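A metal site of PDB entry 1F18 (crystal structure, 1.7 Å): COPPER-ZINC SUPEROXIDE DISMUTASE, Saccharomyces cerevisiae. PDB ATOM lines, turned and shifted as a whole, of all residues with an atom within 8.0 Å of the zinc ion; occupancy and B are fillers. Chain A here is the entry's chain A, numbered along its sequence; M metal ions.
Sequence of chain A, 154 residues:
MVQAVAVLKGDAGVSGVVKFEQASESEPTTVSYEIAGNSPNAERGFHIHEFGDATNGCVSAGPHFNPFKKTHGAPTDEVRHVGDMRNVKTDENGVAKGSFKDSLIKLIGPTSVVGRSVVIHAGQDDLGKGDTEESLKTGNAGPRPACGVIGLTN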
ATOM      1  N   PHE A  46      11.091  -0.623 -13.731  1.00  0.00           N
ATOM      2  CA  PHE A  46      10.936  -1.874 -14.472  1.00  0.00           C
ATOM      3  C   PHE A  46      10.198  -2.840 -13.536  1.00  0.00           C
ATOM      4  O   PHE A  46      10.743  -3.224 -12.501  1.00  0.00           O
ATOM      5  CB  PHE A  46      12.385  -2.313 -14.770  1.00  0.00           C
ATOM      6  CG  PHE A  46      12.522  -3.584 -15.547  1.00  0.00           C
ATOM      7  CD1 PHE A  46      11.923  -3.750 -16.790  1.00  0.00           C
ATOM      8  CD2 PHE A  46      13.346  -4.616 -15.070  1.00  0.00           C
ATOM      9  CE1 PHE A  46      12.127  -4.907 -17.536  1.00  0.00           C
ATOM     10  CE2 PHE A  46      13.565  -5.786 -15.812  1.00  0.00           C
ATOM     11  CZ  PHE A  46      12.956  -5.933 -17.052  1.00  0.00           C
ATOM     12  N   HIS A  47       8.964  -3.226 -13.888  1.00  0.00           N
ATOM     13  CA  HIS A  47       8.175  -4.091 -12.990  1.00  0.00           C
ATOM     14  C   HIS A  47       7.321  -5.143 -13.669  1.00  0.00           C
ATOM     15  O   HIS A  47       7.007  -5.046 -14.839  1.00  0.00           O
ATOM     16  CB  HIS A  47       7.141  -3.246 -12.167  1.00  0.00           C
ATOM     17  CG  HIS A  47       7.648  -1.913 -11.704  1.00  0.00           C
ATOM     18  ND1 HIS A  47       7.193  -0.723 -12.225  1.00  0.00           N
ATOM     19  CD2 HIS A  47       8.596  -1.591 -10.796  1.00  0.00           C
ATOM     20  CE1 HIS A  47       7.847   0.282 -11.669  1.00  0.00           C
ATOM     21  NE2 HIS A  47       8.698  -0.220 -10.796  1.00  0.00           N
ATOM     22  N   ILE A  48       6.864  -6.107 -12.861  1.00  0.00           N
ATOM     23  CA  ILE A  48       5.899  -7.108 -13.309  1.00  0.00           C
ATOM     24  C   ILE A  48       4.539  -6.509 -12.855  1.00  0.00           C
ATOM     25  O   ILE A  48       4.399  -6.051 -11.708  1.00  0.00           O
ATOM     26  CB  ILE A  48       6.024  -8.493 -12.610  1.00  0.00           C
ATOM     27  CG1 ILE A  48       7.458  -9.009 -12.702  1.00  0.00           C
ATOM     28  CG2 ILE A  48       4.994  -9.454 -13.194  1.00  0.00           C
ATOM     29  CD1 ILE A  48       7.905  -9.228 -14.102  1.00  0.00           C
ATOM     30  N   HIS A  49       3.645  -6.357 -13.817  1.00  0.00           N
ATOM     31  CA  HIS A  49       2.297  -5.850 -13.570  1.00  0.00           C
ATOM     32  C   HIS A  49       1.323  -7.038 -13.524  1.00  0.00           C
ATOM     33  O   HIS A  49       1.595  -8.110 -14.090  1.00  0.00           O
ATOM     34  CB  HIS A  49       1.894  -4.780 -14.584  1.00  0.00           C
ATOM     35  CG  HIS A  49       2.550  -3.464 -14.333  1.00  0.00           C
ATOM     36  ND1 HIS A  49       1.839  -2.299 -14.172  1.00  0.00           N
ATOM     37  CD2 HIS A  49       3.856  -3.140 -14.208  1.00  0.00           C
ATOM     38  CE1 HIS A  49       2.692  -1.299 -13.975  1.00  0.00           C
ATOM     39  NE2 HIS A  49       3.925  -1.791 -13.999  1.00  0.00           N
ATOM     40  N   PRO A  63      -2.009  -2.687 -12.171  1.00  0.00           N
ATOM     41  CA  PRO A  63      -1.010  -2.216 -11.210  1.00  0.00           C
ATOM     42  C   PRO A  63       0.127  -3.268 -11.056  1.00  0.00           C
ATOM     43  O   PRO A  63       0.110  -4.331 -11.684  1.00  0.00           O
ATOM     44  CB  PRO A  63      -1.863  -2.078  -9.943  1.00  0.00           C
ATOM     45  CG  PRO A  63      -2.679  -3.314 -10.038  1.00  0.00           C
ATOM     46  CD  PRO A  63      -3.125  -3.364 -11.471  1.00  0.00           C
ATOM     47  N   HIS A  64       1.116  -2.942 -10.237  1.00  0.00           N
ATOM     48  CA  HIS A  64       2.219  -3.879  -9.976  1.00  0.00           C
ATOM     49  C   HIS A  64       1.658  -5.152  -9.351  1.00  0.00           C
ATOM     50  O   HIS A  64       0.714  -5.098  -8.541  1.00  0.00           O
ATOM     51  CB  HIS A  64       3.198  -3.273  -8.997  1.00  0.00           C
ATOM     52  CG  HIS A  64       3.880  -2.043  -9.501  1.00  0.00           C
ATOM     53  ND1 HIS A  64       4.763  -1.328  -8.725  1.00  0.00           N
ATOM     54  CD2 HIS A  64       3.785  -1.381 -10.686  1.00  0.00           C
ATOM     55  CE1 HIS A  64       5.180  -0.261  -9.395  1.00  0.00           C
ATOM     56  NE2 HIS A  64       4.596  -0.273 -10.584  1.00  0.00           N
ATOM     57  N   PHE A  65       2.206  -6.303  -9.778  1.00  0.00           N
ATOM     58  CA  PHE A  65       1.783  -7.604  -9.256  1.00  0.00           C
ATOM     59  C   PHE A  65       2.116  -7.579  -7.743  1.00  0.00           C
ATOM     60  O   PHE A  65       3.272  -7.415  -7.326  1.00  0.00           O
ATOM     61  CB  PHE A  65       2.482  -8.716 -10.027  1.00  0.00           C
ATOM     62  CG  PHE A  65       2.074 -10.104  -9.596  1.00  0.00           C
ATOM     63  CD1 PHE A  65       0.740 -10.415  -9.365  1.00  0.00           C
ATOM     64  CD2 PHE A  65       3.049 -11.090  -9.376  1.00  0.00           C
ATOM     65  CE1 PHE A  65       0.384 -11.706  -8.909  1.00  0.00           C
ATOM     66  CE2 PHE A  65       2.684 -12.364  -8.931  1.00  0.00           C
ATOM     67  CZ  PHE A  65       1.354 -12.668  -8.694  1.00  0.00           C
ATOM     68  N   ASN A  66       1.077  -7.657  -6.914  1.00  0.00           N
ATOM     69  CA  ASN A  66       1.235  -7.526  -5.461  1.00  0.00           C
ATOM     70  C   ASN A  66       0.277  -8.460  -4.729  1.00  0.00           C
ATOM     71  O   ASN A  66      -0.580  -7.999  -3.957  1.00  0.00           O
ATOM     72  CB  ASN A  66       0.843  -6.102  -5.121  1.00  0.00           C
ATOM     73  CG  ASN A  66       1.108  -5.734  -3.690  1.00  0.00           C
ATOM     74  OD1 ASN A  66       1.942  -6.358  -3.007  1.00  0.00           O
ATOM     75  ND2 ASN A  66       0.445  -4.660  -3.240  1.00  0.00           N
ATOM     76  N   LYS A  70       1.550  -5.626  -0.130  1.00  0.00           N
ATOM     77  CA  LYS A  70       2.590  -4.852   0.509  1.00  0.00           C
ATOM     78  C   LYS A  70       2.685  -3.506  -0.224  1.00  0.00           C
ATOM     79  O   LYS A  70       2.034  -3.311  -1.239  1.00  0.00           O
ATOM     80  CB  LYS A  70       3.942  -5.593   0.381  1.00  0.00           C
ATOM     81  CG  LYS A  70       3.966  -7.031   0.919  1.00  0.00           C
ATOM     82  CD  LYS A  70       3.712  -7.059   2.411  1.00  0.00           C
ATOM     83  CE  LYS A  70       4.073  -8.407   3.008  1.00  0.00           C
ATOM     84  NZ  LYS A  70       5.549  -8.711   2.804  1.00  0.00           N
ATOM     85  N   THR A  71       3.482  -2.596   0.293  1.00  0.00           N
ATOM     86  CA  THR A  71       3.714  -1.323  -0.376  1.00  0.00           C
ATOM     87  C   THR A  71       4.874  -1.519  -1.347  1.00  0.00           C
ATOM     88  O   THR A  71       5.654  -2.470  -1.256  1.00  0.00           O
ATOM     89  CB  THR A  71       4.094  -0.184   0.582  1.00  0.00           C
ATOM     90  OG1 THR A  71       5.142  -0.635   1.454  1.00  0.00           O
ATOM     91  CG2 THR A  71       2.864   0.255   1.402  1.00  0.00           C
ATOM     92  N   HIS A  72       4.989  -0.558  -2.264  1.00  0.00           N
ATOM     93  CA  HIS A  72       6.054  -0.537  -3.283  1.00  0.00           C
ATOM     94  C   HIS A  72       7.444  -0.329  -2.624  1.00  0.00           C
ATOM     95  O   HIS A  72       7.616   0.569  -1.792  1.00  0.00           O
ATOM     96  CB  HIS A  72       5.753   0.615  -4.257  1.00  0.00           C
ATOM     97  CG  HIS A  72       6.729   0.692  -5.368  1.00  0.00           C
ATOM     98  ND1 HIS A  72       6.731  -0.226  -6.408  1.00  0.00           N
ATOM     99  CD2 HIS A  72       7.792   1.492  -5.560  1.00  0.00           C
ATOM    100  CE1 HIS A  72       7.781   0.019  -7.178  1.00  0.00           C
ATOM    101  NE2 HIS A  72       8.437   1.055  -6.684  1.00  0.00           N
ATOM    102  N   GLY A  73       8.430  -1.155  -2.993  1.00  0.00           N
ATOM    103  CA  GLY A  73       9.754  -0.998  -2.412  1.00  0.00           C
ATOM    104  C   GLY A  73      10.904  -1.363  -3.348  1.00  0.00           C
ATOM    105  O   GLY A  73      10.680  -1.599  -4.537  1.00  0.00           O
ATOM    106  N   ALA A  74      12.130  -1.303  -2.825  1.00  0.00           N
ATOM    107  CA  ALA A  74      13.353  -1.663  -3.552  1.00  0.00           C
ATOM    108  C   ALA A  74      13.409  -3.219  -3.589  1.00  0.00           C
ATOM    109  O   ALA A  74      12.787  -3.886  -2.757  1.00  0.00           O
ATOM    110  CB  ALA A  74      14.572  -1.066  -2.848  1.00  0.00           C
ATOM    111  N   ARG A  80       7.962  -5.122  -0.279  1.00  0.00           N
ATOM    112  CA  ARG A  80       7.904  -4.729  -1.681  1.00  0.00           C
ATOM    113  C   ARG A  80       6.828  -5.561  -2.379  1.00  0.00           C
ATOM    114  O   ARG A  80       6.284  -6.538  -1.810  1.00  0.00           O
ATOM    115  CB  ARG A  80       9.251  -5.018  -2.384  1.00  0.00           C
ATOM    116  CG  ARG A  80       9.662  -6.489  -2.339  1.00  0.00           C
ATOM    117  CD  ARG A  80      10.875  -6.812  -3.218  1.00  0.00           C
ATOM    118  NE  ARG A  80      10.412  -7.380  -4.471  1.00  0.00           N
ATOM    119  CZ  ARG A  80      11.094  -8.252  -5.191  1.00  0.00           C
ATOM    120  NH1 ARG A  80      12.287  -8.655  -4.759  1.00  0.00           N
ATOM    121  NH2 ARG A  80      10.570  -8.774  -6.314  1.00  0.00           N
ATOM    122  N   HIS A  81       6.439  -5.110  -3.575  1.00  0.00           N
ATOM    123  CA  HIS A  81       5.491  -5.846  -4.383  1.00  0.00           C
ATOM    124  C   HIS A  81       6.322  -6.980  -4.999  1.00  0.00           C
ATOM    125  O   HIS A  81       7.521  -6.832  -5.217  1.00  0.00           O
ATOM    126  CB  HIS A  81       4.981  -4.954  -5.495  1.00  0.00           C
ATOM    127  CG  HIS A  81       4.175  -3.784  -5.005  1.00  0.00           C
ATOM    128  ND1 HIS A  81       4.119  -2.575  -5.681  1.00  0.00           N
ATOM    129  CD2 HIS A  81       3.352  -3.658  -3.942  1.00  0.00           C
ATOM    130  CE1 HIS A  81       3.297  -1.763  -5.045  1.00  0.00           C
ATOM    131  NE2 HIS A  81       2.819  -2.402  -3.992  1.00  0.00           N
ATOM    132  N   VAL A  82       5.715  -8.137  -5.207  1.00  0.00           N
ATOM    133  CA  VAL A  82       6.428  -9.243  -5.855  1.00  0.00           C
ATOM    134  C   VAL A  82       7.037  -8.724  -7.190  1.00  0.00           C
ATOM    135  O   VAL A  82       8.202  -9.032  -7.521  1.00  0.00           O
ATOM    136  CB  VAL A  82       5.417 -10.346  -6.160  1.00  0.00           C
ATOM    137  CG1 VAL A  82       5.962 -11.302  -7.264  1.00  0.00           C
ATOM    138  CG2 VAL A  82       5.051 -11.088  -4.847  1.00  0.00           C
ATOM    139  N   GLY A  83       6.266  -7.893  -7.930  1.00  0.00           N
ATOM    140  CA  GLY A  83       6.721  -7.364  -9.212  1.00  0.00           C
ATOM    141  C   GLY A  83       7.763  -6.254  -9.208  1.00  0.00           C
ATOM    142  O   GLY A  83       8.137  -5.798 -10.276  1.00  0.00           O
ATOM    143  N   ASP A  84       8.253  -5.822  -8.051  1.00  0.00           N
ATOM    144  CA  ASP A  84       9.242  -4.763  -7.964  1.00  0.00           C
ATOM    145  C   ASP A  84      10.665  -5.167  -8.358  1.00  0.00           C
ATOM    146  O   ASP A  84      11.361  -5.834  -7.611  1.00  0.00           O
ATOM    147  CB  ASP A  84       9.238  -4.153  -6.561  1.00  0.00           C
ATOM    148  CG  ASP A  84       7.967  -3.379  -6.272  1.00  0.00           C
ATOM    149  OD1 ASP A  84       7.218  -3.158  -7.237  1.00  0.00           O
ATOM    150  OD2 ASP A  84       7.717  -2.964  -5.108  1.00  0.00           O
ATOM    151  N   MET A  85      11.060  -4.838  -9.576  1.00  0.00           N
ATOM    152  CA  MET A  85      12.422  -5.132 -10.039  1.00  0.00           C
ATOM    153  C   MET A  85      13.285  -3.836  -9.971  1.00  0.00           C
ATOM    154  O   MET A  85      12.807  -2.688  -9.766  1.00  0.00           O
ATOM    155  CB  MET A  85      12.381  -5.730 -11.442  1.00  0.00           C
ATOM    156  CG  MET A  85      11.505  -6.942 -11.541  1.00  0.00           C
ATOM    157  SD  MET A  85      11.571  -7.792 -13.112  1.00  0.00           S
ATOM    158  CE  MET A  85      10.619  -6.680 -14.231  1.00  0.00           C
ATOM    159  N   ASP A 125      12.207   5.016 -10.865  1.00  0.00           N
ATOM    160  CA  ASP A 125      11.413   4.487  -9.744  1.00  0.00           C
ATOM    161  C   ASP A 125      12.114   4.938  -8.444  1.00  0.00           C
ATOM    162  O   ASP A 125      13.306   4.661  -8.258  1.00  0.00           O
ATOM    163  CB  ASP A 125      11.389   2.978  -9.884  1.00  0.00           C
ATOM    164  CG  ASP A 125      10.641   2.254  -8.768  1.00  0.00           C
ATOM    165  OD1 ASP A 125      10.427   2.804  -7.652  1.00  0.00           O
ATOM    166  OD2 ASP A 125      10.290   1.080  -9.024  1.00  0.00           O
ATOM    167  N   LEU A 127      11.720   3.787  -5.555  1.00  0.00           N
ATOM    168  CA  LEU A 127      11.808   2.630  -4.676  1.00  0.00           C
ATOM    169  C   LEU A 127      10.952   2.726  -3.380  1.00  0.00           C
ATOM    170  O   LEU A 127      11.241   2.065  -2.361  1.00  0.00           O
ATOM    171  CB  LEU A 127      13.286   2.370  -4.374  1.00  0.00           C
ATOM    172  CG  LEU A 127      14.162   2.210  -5.650  1.00  0.00           C
ATOM    173  CD1 LEU A 127      15.598   2.023  -5.257  1.00  0.00           C
ATOM    174  CD2 LEU A 127      13.719   1.046  -6.560  1.00  0.00           C
ATOM    175  N   GLY A 128       9.877   3.507  -3.445  1.00  0.00           N
ATOM    176  CA  GLY A 128       8.999   3.688  -2.296  1.00  0.00           C
ATOM    177  C   GLY A 128       9.535   4.671  -1.265  1.00  0.00           C
ATOM    178  O   GLY A 128       8.971   4.773  -0.183  1.00  0.00           O
ATOM    179  N   SER A 135       4.352   7.206  -4.056  1.00  0.00           N
ATOM    180  CA  SER A 135       5.632   6.536  -3.980  1.00  0.00           C
ATOM    181  C   SER A 135       5.427   5.080  -3.515  1.00  0.00           C
ATOM    182  O   SER A 135       6.087   4.158  -4.005  1.00  0.00           O
ATOM    183  CB  SER A 135       6.522   7.261  -2.988  1.00  0.00           C
ATOM    184  OG  SER A 135       7.799   6.623  -2.896  1.00  0.00           O
ATOM    185  N   LEU A 136       4.492   4.886  -2.589  1.00  0.00           N
ATOM    186  CA  LEU A 136       4.195   3.568  -2.035  1.00  0.00           C
ATOM    187  C   LEU A 136       3.314   2.726  -2.934  1.00  0.00           C
ATOM    188  O   LEU A 136       3.049   1.553  -2.632  1.00  0.00           O
ATOM    189  CB  LEU A 136       3.587   3.721  -0.656  1.00  0.00           C
ATOM    190  CG  LEU A 136       4.507   4.355   0.376  1.00  0.00           C
ATOM    191  CD1 LEU A 136       3.705   4.496   1.670  1.00  0.00           C
ATOM    192  CD2 LEU A 136       5.755   3.534   0.633  1.00  0.00           C
ATOM    193  N   LYS A 137       2.939   3.282  -4.088  1.00  0.00           N
ATOM    194  CA  LYS A 137       2.110   2.535  -5.019  1.00  0.00           C
ATOM    195  C   LYS A 137       2.836   2.148  -6.286  1.00  0.00           C
ATOM    196  O   LYS A 137       2.723   0.992  -6.765  1.00  0.00           O
ATOM    197  CB  LYS A 137       0.800   3.317  -5.384  1.00  0.00           C
ATOM    198  CG  LYS A 137       0.064   3.863  -4.159  1.00  0.00           C
ATOM    199  CD  LYS A 137      -1.464   3.763  -4.246  1.00  0.00           C
ATOM    200  CE  LYS A 137      -2.166   4.939  -4.908  1.00  0.00           C
ATOM    201  NZ  LYS A 137      -3.647   4.925  -4.514  1.00  0.00           N
ATOM    202  N   THR A 138       3.513   3.146  -6.881  1.00  0.00           N
ATOM    203  CA  THR A 138       4.210   2.967  -8.165  1.00  0.00           C
ATOM    204  C   THR A 138       5.674   3.368  -8.166  1.00  0.00           C
ATOM    205  O   THR A 138       6.370   3.117  -9.121  1.00  0.00           O
ATOM    206  CB  THR A 138       3.524   3.828  -9.277  1.00  0.00           C
ATOM    207  OG1 THR A 138       3.609   5.220  -8.936  1.00  0.00           O
ATOM    208  CG2 THR A 138       2.073   3.471  -9.434  1.00  0.00           C
ATOM    209  N   GLY A 139       6.151   4.005  -7.097  1.00  0.00           N
ATOM    210  CA  GLY A 139       7.520   4.495  -7.065  1.00  0.00           C
ATOM    211  C   GLY A 139       7.645   5.735  -7.957  1.00  0.00           C
ATOM    212  O   GLY A 139       8.765   6.128  -8.290  1.00  0.00           O
HETATM  213 ZN    ZN M   1       5.685  -1.797  -7.026  1.00  0.00          ZN
HETATM  214 CU    CU M   2       5.528  -0.570 -13.468  1.00  0.00          CU
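A ring nitrogen (NE2) of His 81 sits close to the side-chain amide nitrogen of Asn 66, 3.4 Å away.
N of His 72 is in hydrogen-bond range of O of Leu 136.
N of Gly 73 is in hydrogen-bond range of OD2 of Asp 84, 2.9 Å away.
A ring nitrogen (ND1) of His 47 sits close to a ring nitrogen (NE2) of His 64 (3.1 Å).
NE2 of His 72 is in hydrogen-bond range of OD1 of Asp 125, 2.8 Å away.
O of Asp 84 is in hydrogen-bond range of NH2 of Arg 80.
A ring nitrogen (NE2) of His 81 lies within hydrogen-bond range of the backbone carbonyl oxygen (O) of Lys 70.
The zinc ion is bound by ND1 of His 72 (2.0 Å), ND1 of His 64 (2.0 Å), OD1 of Asp 84 (2.1 Å) and ND1 of His 81 (2.2 Å).
The nearest printed residue that does not touch the zinc ion is Lys 137 (4.1 Å).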
